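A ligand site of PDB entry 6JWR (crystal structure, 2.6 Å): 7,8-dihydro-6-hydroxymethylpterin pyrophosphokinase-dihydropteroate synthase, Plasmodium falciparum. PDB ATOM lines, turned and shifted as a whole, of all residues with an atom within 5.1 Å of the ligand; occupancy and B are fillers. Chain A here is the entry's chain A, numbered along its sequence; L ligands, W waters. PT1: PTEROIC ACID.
Water W4 lies within hydrogen-bond range of OD1 of Asp 575 (2.6 Å), O1 of the ligand (2.9 Å), N of Leu 578 (2.9 Å) and N of Gly 605 (3.0 Å).
SD of Met 529 lies close to N4 of the ligand (3.4 Å).
Residues that only touch the ligand: Phe 580 (3.3 Å), Phe 603 (3.4 Å), Ile 504 (3.5 Å), Pro 438 (3.5 Å), Ser 436 (3.6 Å), Gly 579 (3.6 Å), Ala 437 (3.8 Å) and Val 527 (3.99 Å).
Within 4 Å of the ligand: Ser 436, Ala 437, Pro 438, Asp 482, Asn 502, Ile 504, Val 527, Met 529, Asp 575, Gly 579, Phe 580, Phe 603, Gly 605, Lys 609, Arg 610 and Arg 686.
The nearest printed residue that does not touch the ligand is Met 538 (4.1 Å).
The side-chain amino group (NZ) of Lys 609 lies within hydrogen-bond range of the backbone carbonyl oxygen (O) of Gly 605.
OD2 of Asp 430 lies within salt-bridge range of NE of Arg 686, 2.6 Å away.
The side-chain carboxylate of Asp 482 is in hydrogen-bond range of the side-chain amide nitrogen of Asn 502.
OD1 of Asp 575 lies within hydrogen-bond range of N of Gly 577 (3.0 Å).
N of Arg 686 lies within hydrogen-bond range of O of Ile 604.
The backbone carbonyl oxygen (O) of Leu 578 sits at hydrogen-bond distance from the side-chain amino group (NZ) of Lys 609, at 2.8 Å.
The side-chain amide nitrogen (ND2) of Asn 502 lies within hydrogen-bond range of the side-chain carboxylate (OD2) of Asp 430, at 3.0 Å.
The backbone NH (N) of Asp 482 lies within hydrogen-bond range of the side-chain carboxylate (OD1) of Asp 430.
A nitrogen (N4) of the ligand sits at hydrogen-bond distance from the side-chain carboxylate (OD2) of Asp 575, 2.6 Å away.
The backbone NH (N) of Arg 610 sits at hydrogen-bond distance from an oxygen (O23) of the ligand (3.1 Å).
A nitrogen (N6) of the ligand lies close to the guanidinium group (NH2) of Arg 686 (3.4 Å).
O1 of the ligand sits at hydrogen-bond distance from O of Gly 605 (3.4 Å).
The side-chain amide oxygen (OD1) of Asn 502 lies within hydrogen-bond range of a nitrogen (N11) of the ligand (2.8 Å).
An oxygen (O1) of the ligand is in hydrogen-bond range of the side-chain amino group (NZ) of Lys 609 (2.6 Å).
A nitrogen (N8) of the ligand sits at hydrogen-bond distance from the side-chain carboxylate (OD2) of Asp 482 (2.6 Å).
NH2 of Arg 610 lies within salt-bridge range of O22 of the ligand, 3.0 Å away.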
ATOM      1  N   ASP A 430       2.321   1.481  19.340  1.00  0.00           N
ATOM      2  CA  ASP A 430       3.053   1.864  18.130  1.00  0.00           C
ATOM      3  C   ASP A 430       4.521   1.545  18.360  1.00  0.00           C
ATOM      4  O   ASP A 430       5.170   2.163  19.203  1.00  0.00           O
ATOM      5  CB  ASP A 430       2.843   3.356  17.820  1.00  0.00           C
ATOM      6  CG  ASP A 430       3.426   3.779  16.445  1.00  0.00           C
ATOM      7  OD1 ASP A 430       3.325   3.026  15.441  1.00  0.00           O
ATOM      8  OD2 ASP A 430       3.974   4.919  16.374  1.00  0.00           O
ATOM      9  N   SER A 436      12.408   9.546  14.094  1.00  0.00           N
ATOM     10  CA  SER A 436      12.018  10.645  13.205  1.00  0.00           C
ATOM     11  C   SER A 436      12.204  11.978  13.941  1.00  0.00           C
ATOM     12  O   SER A 436      11.982  13.049  13.366  1.00  0.00           O
ATOM     13  CB  SER A 436      10.563  10.531  12.724  1.00  0.00           C
ATOM     14  OG  SER A 436       9.989   9.242  12.993  1.00  0.00           O
ATOM     15  N   ALA A 437      12.633  11.897  15.203  1.00  0.00           N
ATOM     16  CA  ALA A 437      12.818  13.085  16.046  1.00  0.00           C
ATOM     17  C   ALA A 437      13.784  14.116  15.409  1.00  0.00           C
ATOM     18  O   ALA A 437      14.677  13.731  14.652  1.00  0.00           O
ATOM     19  CB  ALA A 437      13.273  12.667  17.442  1.00  0.00           C
ATOM     20  N   PRO A 438      13.601  15.431  15.694  1.00  0.00           N
ATOM     21  CA  PRO A 438      14.434  16.401  14.967  1.00  0.00           C
ATOM     22  C   PRO A 438      15.931  16.163  15.174  1.00  0.00           C
ATOM     23  O   PRO A 438      16.358  15.865  16.302  1.00  0.00           O
ATOM     24  CB  PRO A 438      14.013  17.756  15.566  1.00  0.00           C
ATOM     25  CG  PRO A 438      12.782  17.478  16.362  1.00  0.00           C
ATOM     26  CD  PRO A 438      12.891  16.066  16.804  1.00  0.00           C
ATOM     27  N   ASP A 482       5.583   1.707  13.257  1.00  0.00           N
ATOM     28  CA  ASP A 482       6.106   2.949  12.720  1.00  0.00           C
ATOM     29  C   ASP A 482       7.290   2.677  11.788  1.00  0.00           C
ATOM     30  O   ASP A 482       8.446   2.750  12.205  1.00  0.00           O
ATOM     31  CB  ASP A 482       6.585   3.797  13.894  1.00  0.00           C
ATOM     32  CG  ASP A 482       6.804   5.246  13.533  1.00  0.00           C
ATOM     33  OD1 ASP A 482       7.213   5.568  12.383  1.00  0.00           O
ATOM     34  OD2 ASP A 482       6.590   6.082  14.439  1.00  0.00           O
ATOM     35  N   ASN A 502       2.063   2.330  10.383  1.00  0.00           N
ATOM     36  CA  ASN A 502       2.218   3.769  10.645  1.00  0.00           C
ATOM     37  C   ASN A 502       3.332   4.242   9.714  1.00  0.00           C
ATOM     38  O   ASN A 502       4.491   4.151  10.037  1.00  0.00           O
ATOM     39  CB  ASN A 502       2.522   4.039  12.123  1.00  0.00           C
ATOM     40  CG  ASN A 502       2.745   5.521  12.423  1.00  0.00           C
ATOM     41  OD1 ASN A 502       2.383   6.387  11.639  1.00  0.00           O
ATOM     42  ND2 ASN A 502       3.325   5.815  13.575  1.00  0.00           N
ATOM     43  N   ILE A 504       4.988   7.215   8.151  1.00  0.00           N
ATOM     44  CA  ILE A 504       5.160   8.654   8.255  1.00  0.00           C
ATOM     45  C   ILE A 504       5.418   9.406   6.944  1.00  0.00           C
ATOM     46  O   ILE A 504       5.498  10.629   6.950  1.00  0.00           O
ATOM     47  CB  ILE A 504       6.190   9.046   9.331  1.00  0.00           C
ATOM     48  CG1 ILE A 504       7.614   8.540   8.966  1.00  0.00           C
ATOM     49  CG2 ILE A 504       5.696   8.578  10.718  1.00  0.00           C
ATOM     50  CD1 ILE A 504       8.729   9.301   9.656  1.00  0.00           C
ATOM     51  N   VAL A 527      -1.951   4.259   8.903  1.00  0.00           N
ATOM     52  CA  VAL A 527      -1.871   5.679   9.220  1.00  0.00           C
ATOM     53  C   VAL A 527      -1.074   6.393   8.123  1.00  0.00           C
ATOM     54  O   VAL A 527       0.035   5.975   7.807  1.00  0.00           O
ATOM     55  CB  VAL A 527      -1.187   5.937  10.592  1.00  0.00           C
ATOM     56  CG1 VAL A 527      -1.358   7.394  11.033  1.00  0.00           C
ATOM     57  CG2 VAL A 527      -1.758   5.013  11.636  1.00  0.00           C
ATOM     58  N   MET A 529       0.657   9.932   7.298  1.00  0.00           N
ATOM     59  CA  MET A 529       1.102  11.148   8.003  1.00  0.00           C
ATOM     60  C   MET A 529       1.678  12.212   7.047  1.00  0.00           C
ATOM     61  O   MET A 529       2.338  11.860   6.052  1.00  0.00           O
ATOM     62  CB  MET A 529       2.128  10.821   9.085  1.00  0.00           C
ATOM     63  CG  MET A 529       2.230  11.912  10.132  1.00  0.00           C
ATOM     64  SD  MET A 529       3.772  11.968  11.080  1.00  0.00           S
ATOM     65  CE  MET A 529       4.865  12.641   9.804  1.00  0.00           C
ATOM     66  N   MET A 538      13.698  19.092   7.774  1.00  0.00           N
ATOM     67  CA  MET A 538      12.259  19.424   7.941  1.00  0.00           C
ATOM     68  C   MET A 538      11.971  20.792   8.563  1.00  0.00           C
ATOM     69  O   MET A 538      11.040  21.446   8.140  1.00  0.00           O
ATOM     70  CB  MET A 538      11.499  18.320   8.662  1.00  0.00           C
ATOM     71  CG  MET A 538      11.915  18.105  10.090  1.00  0.00           C
ATOM     72  SD  MET A 538      10.875  16.808  10.715  1.00  0.00           S
ATOM     73  CE  MET A 538      11.371  16.805  12.450  1.00  0.00           C
ATOM     74  N   ASP A 575      -3.160  11.646   9.702  1.00  0.00           N
ATOM     75  CA  ASP A 575      -2.296  12.306  10.682  1.00  0.00           C
ATOM     76  C   ASP A 575      -1.626  13.558  10.065  1.00  0.00           C
ATOM     77  O   ASP A 575      -0.978  13.523   8.998  1.00  0.00           O
ATOM     78  CB  ASP A 575      -1.271  11.310  11.251  1.00  0.00           C
ATOM     79  CG  ASP A 575      -0.460  11.870  12.451  1.00  0.00           C
ATOM     80  OD1 ASP A 575      -0.560  13.086  12.796  1.00  0.00           O
ATOM     81  OD2 ASP A 575       0.303  11.068  13.053  1.00  0.00           O
ATOM     82  N   GLY A 577       0.829  15.189  11.126  1.00  0.00           N
ATOM     83  CA  GLY A 577       2.264  15.237  11.373  1.00  0.00           C
ATOM     84  C   GLY A 577       2.750  16.467  12.136  1.00  0.00           C
ATOM     85  O   GLY A 577       3.536  17.250  11.618  1.00  0.00           O
ATOM     86  N   LEU A 578       2.300  16.616  13.383  1.00  0.00           N
ATOM     87  CA  LEU A 578       2.721  17.709  14.227  1.00  0.00           C
ATOM     88  C   LEU A 578       4.243  17.704  14.427  1.00  0.00           C
ATOM     89  O   LEU A 578       4.842  16.642  14.639  1.00  0.00           O
ATOM     90  CB  LEU A 578       1.998  17.647  15.579  1.00  0.00           C
ATOM     91  CG  LEU A 578       0.469  17.890  15.617  1.00  0.00           C
ATOM     92  CD1 LEU A 578      -0.115  17.486  16.959  1.00  0.00           C
ATOM     93  CD2 LEU A 578       0.114  19.332  15.276  1.00  0.00           C
ATOM     94  N   GLY A 579       4.872  18.863  14.339  1.00  0.00           N
ATOM     95  CA  GLY A 579       6.320  18.962  14.489  1.00  0.00           C
ATOM     96  C   GLY A 579       7.159  18.578  13.278  1.00  0.00           C
ATOM     97  O   GLY A 579       8.354  18.745  13.297  1.00  0.00           O
ATOM     98  N   PHE A 580       6.517  18.075  12.220  1.00  0.00           N
ATOM     99  CA  PHE A 580       7.212  17.666  11.005  1.00  0.00           C
ATOM    100  C   PHE A 580       7.001  18.732   9.944  1.00  0.00           C
ATOM    101  O   PHE A 580       5.913  18.780   9.334  1.00  0.00           O
ATOM    102  CB  PHE A 580       6.612  16.381  10.453  1.00  0.00           C
ATOM    103  CG  PHE A 580       6.933  15.131  11.217  1.00  0.00           C
ATOM    104  CD1 PHE A 580       6.111  14.700  12.263  1.00  0.00           C
ATOM    105  CD2 PHE A 580       8.003  14.310  10.825  1.00  0.00           C
ATOM    106  CE1 PHE A 580       6.371  13.507  12.925  1.00  0.00           C
ATOM    107  CE2 PHE A 580       8.261  13.111  11.471  1.00  0.00           C
ATOM    108  CZ  PHE A 580       7.441  12.708  12.531  1.00  0.00           C
ATOM    109  N   PHE A 603      -5.565  10.494  13.639  1.00  0.00           N
ATOM    110  CA  PHE A 603      -4.480   9.990  14.471  1.00  0.00           C
ATOM    111  C   PHE A 603      -3.534  11.179  14.642  1.00  0.00           C
ATOM    112  O   PHE A 603      -3.159  11.808  13.663  1.00  0.00           O
ATOM    113  CB  PHE A 603      -3.796   8.856  13.695  1.00  0.00           C
ATOM    114  CG  PHE A 603      -2.730   8.108  14.437  1.00  0.00           C
ATOM    115  CD1 PHE A 603      -1.465   8.663  14.639  1.00  0.00           C
ATOM    116  CD2 PHE A 603      -2.942   6.782  14.817  1.00  0.00           C
ATOM    117  CE1 PHE A 603      -0.435   7.934  15.265  1.00  0.00           C
ATOM    118  CE2 PHE A 603      -1.941   6.057  15.471  1.00  0.00           C
ATOM    119  CZ  PHE A 603      -0.684   6.633  15.691  1.00  0.00           C
ATOM    120  N   ILE A 604      -3.192  11.564  15.865  1.00  0.00           N
ATOM    121  CA  ILE A 604      -2.200  12.633  16.058  1.00  0.00           C
ATOM    122  C   ILE A 604      -1.145  12.261  17.104  1.00  0.00           C
ATOM    123  O   ILE A 604      -1.422  11.482  18.016  1.00  0.00           O
ATOM    124  CB  ILE A 604      -2.827  14.011  16.375  1.00  0.00           C
ATOM    125  CG1 ILE A 604      -3.363  14.077  17.822  1.00  0.00           C
ATOM    126  CG2 ILE A 604      -3.905  14.364  15.353  1.00  0.00           C
ATOM    127  CD1 ILE A 604      -3.874  15.445  18.191  1.00  0.00           C
ATOM    128  N   GLY A 605       0.055  12.808  16.943  1.00  0.00           N
ATOM    129  CA  GLY A 605       1.120  12.670  17.909  1.00  0.00           C
ATOM    130  C   GLY A 605       1.672  14.027  18.327  1.00  0.00           C
ATOM    131  O   GLY A 605       2.409  14.668  17.572  1.00  0.00           O
ATOM    132  N   ARG A 608       5.347  15.153  23.802  1.00  0.00           N
ATOM    133  CA  ARG A 608       6.697  15.616  24.166  1.00  0.00           C
ATOM    134  C   ARG A 608       7.380  16.430  23.095  1.00  0.00           C
ATOM    135  O   ARG A 608       8.601  16.585  23.128  1.00  0.00           O
ATOM    136  CB  ARG A 608       7.624  14.468  24.607  1.00  0.00           C
ATOM    137  CG  ARG A 608       7.171  13.777  25.864  1.00  0.00           C
ATOM    138  CD  ARG A 608       8.115  12.636  26.206  1.00  0.00           C
ATOM    139  NE  ARG A 608       7.658  11.846  27.339  1.00  0.00           N
ATOM    140  CZ  ARG A 608       8.393  10.904  27.930  1.00  0.00           C
ATOM    141  NH1 ARG A 608       9.628  10.643  27.506  1.00  0.00           N
ATOM    142  NH2 ARG A 608       7.895  10.227  28.975  1.00  0.00           N
ATOM    143  N   LYS A 609       6.617  16.949  22.136  1.00  0.00           N
ATOM    144  CA  LYS A 609       7.254  17.695  21.052  1.00  0.00           C
ATOM    145  C   LYS A 609       7.610  19.095  21.491  1.00  0.00           C
ATOM    146  O   LYS A 609       7.018  19.633  22.431  1.00  0.00           O
ATOM    147  CB  LYS A 609       6.431  17.642  19.756  1.00  0.00           C
ATOM    148  CG  LYS A 609       6.290  16.213  19.257  1.00  0.00           C
ATOM    149  CD  LYS A 609       5.678  16.115  17.882  1.00  0.00           C
ATOM    150  CE  LYS A 609       5.689  14.652  17.477  1.00  0.00           C
ATOM    151  NZ  LYS A 609       4.838  14.437  16.303  1.00  0.00           N
ATOM    152  N   ARG A 610       8.607  19.667  20.817  1.00  0.00           N
ATOM    153  CA  ARG A 610       9.120  20.996  21.095  1.00  0.00           C
ATOM    154  C   ARG A 610       8.053  22.062  21.191  1.00  0.00           C
ATOM    155  O   ARG A 610       8.150  22.923  22.029  1.00  0.00           O
ATOM    156  CB  ARG A 610      10.193  21.390  20.056  1.00  0.00           C
ATOM    157  CG  ARG A 610      11.471  20.560  20.110  1.00  0.00           C
ATOM    158  CD  ARG A 610      12.318  20.738  18.859  1.00  0.00           C
ATOM    159  NE  ARG A 610      11.607  20.369  17.621  1.00  0.00           N
ATOM    160  CZ  ARG A 610      11.986  20.690  16.381  1.00  0.00           C
ATOM    161  NH1 ARG A 610      13.083  21.409  16.160  1.00  0.00           N
ATOM    162  NH2 ARG A 610      11.252  20.288  15.358  1.00  0.00           N
ATOM    163  N   ARG A 686      -1.210   9.470  19.958  1.00  0.00           N
ATOM    164  CA  ARG A 686       0.052   8.722  20.056  1.00  0.00           C
ATOM    165  C   ARG A 686       0.851   9.309  21.211  1.00  0.00           C
ATOM    166  O   ARG A 686       1.359  10.422  21.087  1.00  0.00           O
ATOM    167  CB  ARG A 686       0.811   8.821  18.723  1.00  0.00           C
ATOM    168  CG  ARG A 686       1.987   7.865  18.595  1.00  0.00           C
ATOM    169  CD  ARG A 686       2.772   8.015  17.282  1.00  0.00           C
ATOM    170  NE  ARG A 686       4.072   7.351  17.381  1.00  0.00           N
ATOM    171  CZ  ARG A 686       5.185   7.930  17.843  1.00  0.00           C
ATOM    172  NH1 ARG A 686       6.306   7.228  17.917  1.00  0.00           N
ATOM    173  NH2 ARG A 686       5.181   9.204  18.208  1.00  0.00           N
HETATM  174  C2  PT1 L   1       3.613  11.360  14.681  1.00  0.00           C
HETATM  175  C3  PT1 L   1       4.907  10.685  14.922  1.00  0.00           C
HETATM  176  C5  PT1 L   1       5.059   9.297  14.407  1.00  0.00           C
HETATM  177  N6  PT1 L   1       5.917  11.297  15.578  1.00  0.00           N
HETATM  178  C7  PT1 L   1       2.868   9.404  13.566  1.00  0.00           C
HETATM  179  N9  PT1 L   1       4.026   8.681  13.755  1.00  0.00           N
HETATM  180  C10 PT1 L   1       7.062  10.624  15.762  1.00  0.00           C
HETATM  181  N11 PT1 L   1       1.845   8.838  12.919  1.00  0.00           N
HETATM  182  C12 PT1 L   1       7.205   9.317  15.285  1.00  0.00           C
HETATM  183  C21 PT1 L   1       9.448  17.611  17.529  1.00  0.00           C
HETATM  184  O22 PT1 L   1       9.250  18.643  16.810  1.00  0.00           O
HETATM  185  O1  PT1 L   1       3.389  12.610  15.109  1.00  0.00           O
HETATM  186  N4  PT1 L   1       2.677  10.682  14.010  1.00  0.00           N
HETATM  187  N8  PT1 L   1       6.225   8.682  14.634  1.00  0.00           N
HETATM  188  C13 PT1 L   1       8.197  11.295  16.485  1.00  0.00           C
HETATM  189  N14 PT1 L   1       8.706  12.341  15.607  1.00  0.00           N
HETATM  190  C15 PT1 L   1       8.885  13.623  16.034  1.00  0.00           C
HETATM  191  C16 PT1 L   1       9.299  13.859  17.355  1.00  0.00           C
HETATM  192  C17 PT1 L   1       8.679  14.708  15.151  1.00  0.00           C
HETATM  193  C18 PT1 L   1       9.461  15.158  17.821  1.00  0.00           C
HETATM  194  C19 PT1 L   1       8.849  16.010  15.640  1.00  0.00           C
HETATM  195  C20 PT1 L   1       9.253  16.238  16.965  1.00  0.00           C
HETATM  196  O23 PT1 L   1       9.769  17.689  18.743  1.00  0.00           O
HETATM  197  O   HOH W   1       8.477   9.421  19.362  1.00  0.00           O
HETATM  198  O   HOH W   2       8.876  12.123  20.344  1.00  0.00           O
HETATM  199  O   HOH W   3       7.125  20.361  17.479  1.00  0.00           O
HETATM  200  O   HOH W   4       1.095  14.232  14.509  1.00  0.00           O
